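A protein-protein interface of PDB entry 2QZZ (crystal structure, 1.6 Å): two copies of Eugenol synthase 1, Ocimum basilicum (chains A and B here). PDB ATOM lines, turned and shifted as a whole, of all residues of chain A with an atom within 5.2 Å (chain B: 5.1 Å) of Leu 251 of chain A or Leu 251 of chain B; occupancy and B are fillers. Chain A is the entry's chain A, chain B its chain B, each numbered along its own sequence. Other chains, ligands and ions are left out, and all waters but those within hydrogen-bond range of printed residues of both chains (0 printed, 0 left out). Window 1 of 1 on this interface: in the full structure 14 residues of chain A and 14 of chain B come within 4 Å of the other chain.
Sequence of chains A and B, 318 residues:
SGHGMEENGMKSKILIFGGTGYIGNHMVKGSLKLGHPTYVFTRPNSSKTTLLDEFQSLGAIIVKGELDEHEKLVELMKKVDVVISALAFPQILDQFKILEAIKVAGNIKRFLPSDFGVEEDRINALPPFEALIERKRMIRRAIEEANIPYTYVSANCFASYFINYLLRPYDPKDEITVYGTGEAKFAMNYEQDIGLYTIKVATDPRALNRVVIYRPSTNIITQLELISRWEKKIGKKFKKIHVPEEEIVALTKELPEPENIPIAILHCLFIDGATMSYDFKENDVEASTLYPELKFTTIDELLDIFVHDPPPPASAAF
The side-chain carboxylate (OE2) of Glu 247 of chain A sits close to the side-chain carboxylate (OE2) of Glu 247 of chain B (2.4 Å).
Glu 247 of chain A touches its own counterpart, Glu 247 of chain B.
Leu 251 of chain A touches Glu 247 of chain B, but with the chains exchanged Glu 247 of chain A does not touch Leu 251 of chain B (4.4 Å).
Leu 251 of chain B touches its own counterpart, Leu 251 of chain A.
Glu 254 of chain A touches Glu 247 of chain B, but with the chains exchanged Glu 247 of chain A does not touch Glu 254 of chain B (4.2 Å).
Positions printed for both chains: 247, 248, 249, 250, 251, 252, 253, 254, 255, 260 and 263.
Of the 11 printed residues of chain B, 2 touch a printed residue of chain A.
Hydrophobic or aromatic side chains of chain B that line the printed part of chain A: Leu 251.
Printed residues of chain A that touch a printed residue of chain B: Glu 247, Leu 251 and Glu 254.
Hydrophobic or aromatic side chains of chain A within 4 Å of the printed part of chain B: Leu 251.
Among the printed residues, no Asp or Glu carboxylate lies within 4 Å of a Lys or Arg side-chain nitrogen of the other chain.
Of the printed residues of chain B, Glu 247 of chain A touches Glu 247 (2.4 Å).
Asn 260 of chain A touches none of the printed residues of chain B.
Printed residues of chain A within 4 Å of Glu 247 of chain B: Glu 247 (2.4 Å), Leu 251 (3.9 Å) and Glu 254 (3.5 Å).
Leu 251 of chain B touches one residue of chain A.
The nearest printed residue of chain B that does not touch Leu 251 of chain A is Leu 255 of chain B (5.6 Å).
The nearest residue of chain A that does not touch Leu 251 of chain B is Glu 247 of chain A (4.4 Å).
Glu 247 of chain B touches Leu 251 of chain A (OE2 to CD2, 3.9 Å).
CD1 of Leu 251 of chain A touches CD2 of Leu 251 of chain B (3.6 Å).
Glu 247 of chain B touches Glu 254 of chain A (CG to OE2, 3.5 Å).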
ATOM      1  N   GLU A 247     -19.061  22.431  21.754  1.00  0.00           N
ATOM      2  CA  GLU A 247     -18.472  22.344  23.080  1.00  0.00           C
ATOM      3  C   GLU A 247     -17.894  23.700  23.479  1.00  0.00           C
ATOM      4  O   GLU A 247     -18.106  24.185  24.592  1.00  0.00           O
ATOM      5  CB  GLU A 247     -17.369  21.286  23.084  1.00  0.00           C
ATOM      6  CG  GLU A 247     -16.689  21.135  24.418  1.00  0.00           C
ATOM      7  CD  GLU A 247     -17.683  20.878  25.520  1.00  0.00           C
ATOM      8  OE1 GLU A 247     -18.309  19.798  25.520  1.00  0.00           O
ATOM      9  OE2 GLU A 247     -17.848  21.768  26.380  1.00  0.00           O
ATOM     10  N   ILE A 248     -17.158  24.304  22.556  1.00  0.00           N
ATOM     11  CA  ILE A 248     -16.544  25.600  22.793  1.00  0.00           C
ATOM     12  C   ILE A 248     -17.614  26.661  23.042  1.00  0.00           C
ATOM     13  O   ILE A 248     -17.483  27.488  23.945  1.00  0.00           O
ATOM     14  CB  ILE A 248     -15.661  25.995  21.590  1.00  0.00           C
ATOM     15  CG1 ILE A 248     -14.465  25.039  21.512  1.00  0.00           C
ATOM     16  CG2 ILE A 248     -15.203  27.440  21.715  1.00  0.00           C
ATOM     17  CD1 ILE A 248     -13.549  25.273  20.331  1.00  0.00           C
ATOM     18  N   VAL A 249     -18.677  26.627  22.248  1.00  0.00           N
ATOM     19  CA  VAL A 249     -19.762  27.589  22.400  1.00  0.00           C
ATOM     20  C   VAL A 249     -20.410  27.466  23.779  1.00  0.00           C
ATOM     21  O   VAL A 249     -20.665  28.470  24.445  1.00  0.00           O
ATOM     22  CB  VAL A 249     -20.841  27.382  21.315  1.00  0.00           C
ATOM     23  CG1 VAL A 249     -22.036  28.292  21.582  1.00  0.00           C
ATOM     24  CG2 VAL A 249     -20.251  27.669  19.942  1.00  0.00           C
ATOM     25  N   ALA A 250     -20.670  26.234  24.205  1.00  0.00           N
ATOM     26  CA  ALA A 250     -21.290  25.986  25.504  1.00  0.00           C
ATOM     27  C   ALA A 250     -20.488  26.615  26.645  1.00  0.00           C
ATOM     28  O   ALA A 250     -21.050  27.268  27.530  1.00  0.00           O
ATOM     29  CB  ALA A 250     -21.428  24.481  25.734  1.00  0.00           C
ATOM     30  N   LEU A 251     -19.173  26.415  26.615  1.00  0.00           N
ATOM     31  CA  LEU A 251     -18.279  26.943  27.645  1.00  0.00           C
ATOM     32  C   LEU A 251     -18.319  28.462  27.794  1.00  0.00           C
ATOM     33  O   LEU A 251     -18.256  28.981  28.907  1.00  0.00           O
ATOM     34  CB  LEU A 251     -16.839  26.500  27.366  1.00  0.00           C
ATOM     35  CG  LEU A 251     -16.542  25.000  27.440  1.00  0.00           C
ATOM     36  CD1 LEU A 251     -15.135  24.724  26.940  1.00  0.00           C
ATOM     37  CD2 LEU A 251     -16.704  24.522  28.870  1.00  0.00           C
ATOM     38  N   THR A 252     -18.421  29.183  26.680  1.00  0.00           N
ATOM     39  CA  THR A 252     -18.456  30.641  26.738  1.00  0.00           C
ATOM     40  C   THR A 252     -19.677  31.137  27.500  1.00  0.00           C
ATOM     41  O   THR A 252     -19.695  32.268  27.990  1.00  0.00           O
ATOM     42  CB  THR A 252     -18.493  31.268  25.330  1.00  0.00           C
ATOM     43  OG1 THR A 252     -19.741  30.956  24.698  1.00  0.00           O
ATOM     44  CG2 THR A 252     -17.354  30.730  24.480  1.00  0.00           C
ATOM     45  N   LYS A 253     -20.691  30.284  27.604  1.00  0.00           N
ATOM     46  CA  LYS A 253     -21.929  30.633  28.296  1.00  0.00           C
ATOM     47  C   LYS A 253     -21.950  30.218  29.765  1.00  0.00           C
ATOM     48  O   LYS A 253     -22.663  30.817  30.570  1.00  0.00           O
ATOM     49  CB  LYS A 253     -23.121  29.979  27.585  1.00  0.00           C
ATOM     50  CG  LYS A 253     -23.259  30.337  26.116  1.00  0.00           C
ATOM     51  CD  LYS A 253     -24.387  29.544  25.466  1.00  0.00           C
ATOM     52  CE  LYS A 253     -24.476  29.827  23.976  1.00  0.00           C
ATOM     53  NZ  LYS A 253     -25.537  29.007  23.326  1.00  0.00           N
ATOM     54  N   GLU A 254     -21.175  29.195  30.107  1.00  0.00           N
ATOM     55  CA  GLU A 254     -21.152  28.695  31.478  1.00  0.00           C
ATOM     56  C   GLU A 254     -19.952  29.103  32.321  1.00  0.00           C
ATOM     57  O   GLU A 254     -20.066  29.288  33.535  1.00  0.00           O
ATOM     58  CB  GLU A 254     -21.279  27.171  31.474  1.00  0.00           C
ATOM     59  CG  GLU A 254     -20.579  26.486  30.306  1.00  0.00           C
ATOM     60  CD  GLU A 254     -20.936  25.014  30.179  1.00  0.00           C
ATOM     61  OE1 GLU A 254     -22.139  24.689  30.246  1.00  0.00           O
ATOM     62  OE2 GLU A 254     -20.021  24.185  29.998  1.00  0.00           O
ATOM     63  N   LEU A 255     -18.799  29.253  31.682  1.00  0.00           N
ATOM     64  CA  LEU A 255     -17.595  29.638  32.422  1.00  0.00           C
ATOM     65  C   LEU A 255     -17.678  31.117  32.799  1.00  0.00           C
ATOM     66  O   LEU A 255     -18.315  31.898  32.114  1.00  0.00           O
ATOM     67  CB  LEU A 255     -16.355  29.386  31.584  1.00  0.00           C
ATOM     68  CG  LEU A 255     -16.059  27.935  31.181  1.00  0.00           C
ATOM     69  CD1 LEU A 255     -14.804  27.909  30.332  1.00  0.00           C
ATOM     70  CD2 LEU A 255     -15.888  27.075  32.426  1.00  0.00           C
ATOM     71  N   ASN A 260     -13.901  32.766  30.071  1.00  0.00           N
ATOM     72  CA  ASN A 260     -14.641  32.569  28.829  1.00  0.00           C
ATOM     73  C   ASN A 260     -14.198  33.427  27.648  1.00  0.00           C
ATOM     74  O   ASN A 260     -14.615  33.181  26.520  1.00  0.00           O
ATOM     75  CB  ASN A 260     -16.151  32.742  29.064  1.00  0.00           C
ATOM     76  CG  ASN A 260     -16.536  34.157  29.452  1.00  0.00           C
ATOM     77  OD1 ASN A 260     -15.688  35.038  29.589  1.00  0.00           O
ATOM     78  ND2 ASN A 260     -17.833  34.381  29.630  1.00  0.00           N
ATOM     79  N   ILE A 263     -11.713  31.471  25.230  1.00  0.00           N
ATOM     80  CA  ILE A 263     -12.523  30.463  24.561  1.00  0.00           C
ATOM     81  C   ILE A 263     -13.310  31.095  23.410  1.00  0.00           C
ATOM     82  O   ILE A 263     -13.327  30.572  22.299  1.00  0.00           O
ATOM     83  CB  ILE A 263     -13.495  29.784  25.564  1.00  0.00           C
ATOM     84  CG1 ILE A 263     -12.691  29.057  26.646  1.00  0.00           C
ATOM     85  CG2 ILE A 263     -14.390  28.784  24.846  1.00  0.00           C
ATOM     86  CD1 ILE A 263     -11.809  27.945  26.109  1.00  0.00           C
ATOM     87  N   GLU B 247     -19.113  17.394  31.686  1.00  0.00           N
ATOM     88  CA  GLU B 247     -18.525  18.454  30.885  1.00  0.00           C
ATOM     89  C   GLU B 247     -17.085  18.706  31.345  1.00  0.00           C
ATOM     90  O   GLU B 247     -16.156  18.797  30.539  1.00  0.00           O
ATOM     91  CB  GLU B 247     -19.366  19.722  31.047  1.00  0.00           C
ATOM     92  CG  GLU B 247     -18.847  20.901  30.282  1.00  0.00           C
ATOM     93  CD  GLU B 247     -18.562  20.543  28.849  1.00  0.00           C
ATOM     94  OE1 GLU B 247     -19.501  20.103  28.151  1.00  0.00           O
ATOM     95  OE2 GLU B 247     -17.398  20.689  28.427  1.00  0.00           O
ATOM     96  N   ILE B 248     -16.915  18.817  32.656  1.00  0.00           N
ATOM     97  CA  ILE B 248     -15.607  19.048  33.252  1.00  0.00           C
ATOM     98  C   ILE B 248     -14.650  17.901  32.916  1.00  0.00           C
ATOM     99  O   ILE B 248     -13.508  18.123  32.522  1.00  0.00           O
ATOM    100  CB  ILE B 248     -15.743  19.189  34.787  1.00  0.00           C
ATOM    101  CG1 ILE B 248     -16.525  20.463  35.122  1.00  0.00           C
ATOM    102  CG2 ILE B 248     -14.374  19.185  35.444  1.00  0.00           C
ATOM    103  CD1 ILE B 248     -15.846  21.742  34.675  1.00  0.00           C
ATOM    104  N   VAL B 249     -15.131  16.673  33.061  1.00  0.00           N
ATOM    105  CA  VAL B 249     -14.318  15.495  32.774  1.00  0.00           C
ATOM    106  C   VAL B 249     -13.848  15.461  31.318  1.00  0.00           C
ATOM    107  O   VAL B 249     -12.674  15.201  31.042  1.00  0.00           O
ATOM    108  CB  VAL B 249     -15.104  14.201  33.094  1.00  0.00           C
ATOM    109  CG1 VAL B 249     -14.330  12.977  32.614  1.00  0.00           C
ATOM    110  CG2 VAL B 249     -15.350  14.114  34.593  1.00  0.00           C
ATOM    111  N   ALA B 250     -14.761  15.723  30.389  1.00  0.00           N
ATOM    112  CA  ALA B 250     -14.413  15.721  28.971  1.00  0.00           C
ATOM    113  C   ALA B 250     -13.289  16.717  28.694  1.00  0.00           C
ATOM    114  O   ALA B 250     -12.337  16.411  27.973  1.00  0.00           O
ATOM    115  CB  ALA B 250     -15.641  16.065  28.130  1.00  0.00           C
ATOM    116  N   LEU B 251     -13.400  17.906  29.276  1.00  0.00           N
ATOM    117  CA  LEU B 251     -12.410  18.960  29.090  1.00  0.00           C
ATOM    118  C   LEU B 251     -10.994  18.558  29.497  1.00  0.00           C
ATOM    119  O   LEU B 251     -10.026  18.906  28.825  1.00  0.00           O
ATOM    120  CB  LEU B 251     -12.826  20.209  29.873  1.00  0.00           C
ATOM    121  CG  LEU B 251     -14.081  20.934  29.385  1.00  0.00           C
ATOM    122  CD1 LEU B 251     -14.487  22.006  30.386  1.00  0.00           C
ATOM    123  CD2 LEU B 251     -13.807  21.549  28.026  1.00  0.00           C
ATOM    124  N   THR B 252     -10.868  17.825  30.599  1.00  0.00           N
ATOM    125  CA  THR B 252      -9.549  17.408  31.065  1.00  0.00           C
ATOM    126  C   THR B 252      -8.857  16.474  30.079  1.00  0.00           C
ATOM    127  O   THR B 252      -7.643  16.298  30.137  1.00  0.00           O
ATOM    128  CB  THR B 252      -9.626  16.676  32.421  1.00  0.00           C
ATOM    129  OG1 THR B 252     -10.331  15.437  32.260  1.00  0.00           O
ATOM    130  CG2 THR B 252     -10.348  17.534  33.451  1.00  0.00           C
ATOM    131  N   LYS B 253      -9.631  15.884  29.174  1.00  0.00           N
ATOM    132  CA  LYS B 253      -9.090  14.948  28.195  1.00  0.00           C
ATOM    133  C   LYS B 253      -8.824  15.593  26.841  1.00  0.00           C
ATOM    134  O   LYS B 253      -8.020  15.090  26.055  1.00  0.00           O
ATOM    135  CB  LYS B 253     -10.062  13.781  27.994  1.00  0.00           C
ATOM    136  CG  LYS B 253     -10.402  12.999  29.258  1.00  0.00           C
ATOM    137  CD  LYS B 253     -11.509  11.985  28.985  1.00  0.00           C
ATOM    138  CE  LYS B 253     -11.923  11.249  30.250  1.00  0.00           C
ATOM    139  NZ  LYS B 253     -13.067  10.326  30.005  1.00  0.00           N
ATOM    140  N   GLU B 254      -9.498  16.705  26.572  1.00  0.00           N
ATOM    141  CA  GLU B 254      -9.363  17.387  25.285  1.00  0.00           C
ATOM    142  C   GLU B 254      -8.467  18.612  25.313  1.00  0.00           C
ATOM    143  O   GLU B 254      -7.704  18.850  24.377  1.00  0.00           O
ATOM    144  CB  GLU B 254     -10.742  17.803  24.783  1.00  0.00           C
ATOM    145  CG  GLU B 254     -11.805  16.750  24.984  1.00  0.00           C
ATOM    146  CD  GLU B 254     -13.183  17.251  24.625  1.00  0.00           C
ATOM    147  OE1 GLU B 254     -13.468  18.442  24.873  1.00  0.00           O
ATOM    148  OE2 GLU B 254     -13.995  16.454  24.109  1.00  0.00           O
ATOM    149  N   LEU B 255      -8.584  19.398  26.376  1.00  0.00           N
ATOM    150  CA  LEU B 255      -7.803  20.619  26.505  1.00  0.00           C
ATOM    151  C   LEU B 255      -6.319  20.351  26.737  1.00  0.00           C
ATOM    152  O   LEU B 255      -5.937  19.350  27.348  1.00  0.00           O
ATOM    153  CB  LEU B 255      -8.360  21.486  27.638  1.00  0.00           C
ATOM    154  CG  LEU B 255      -9.746  22.114  27.445  1.00  0.00           C
ATOM    155  CD1 LEU B 255     -10.103  22.940  28.672  1.00  0.00           C
ATOM    156  CD2 LEU B 255      -9.750  22.990  26.199  1.00  0.00           C
ATOM    157  N   ASN B 260      -5.701  22.099  31.251  1.00  0.00           N
ATOM    158  CA  ASN B 260      -6.507  21.036  31.840  1.00  0.00           C
ATOM    159  C   ASN B 260      -6.264  20.744  33.314  1.00  0.00           C
ATOM    160  O   ASN B 260      -7.025  19.997  33.921  1.00  0.00           O
ATOM    161  CB  ASN B 260      -6.365  19.737  31.032  1.00  0.00           C
ATOM    162  CG  ASN B 260      -4.961  19.182  31.051  1.00  0.00           C
ATOM    163  OD1 ASN B 260      -4.126  19.594  31.852  1.00  0.00           O
ATOM    164  ND2 ASN B 260      -4.695  18.226  30.170  1.00  0.00           N
ATOM    165  N   ILE B 263      -8.855  22.570  35.698  1.00  0.00           N
ATOM    166  CA  ILE B 263     -10.132  21.900  35.482  1.00  0.00           C
ATOM    167  C   ILE B 263     -10.196  20.596  36.287  1.00  0.00           C
ATOM    168  O   ILE B 263     -11.197  20.310  36.939  1.00  0.00           O
ATOM    169  CB  ILE B 263     -10.355  21.615  33.976  1.00  0.00           C
ATOM    170  CG1 ILE B 263     -10.480  22.938  33.218  1.00  0.00           C
ATOM    171  CG2 ILE B 263     -11.618  20.789  33.772  1.00  0.00           C
ATOM    172  CD1 ILE B 263     -11.685  23.769  33.626  1.00  0.00           C
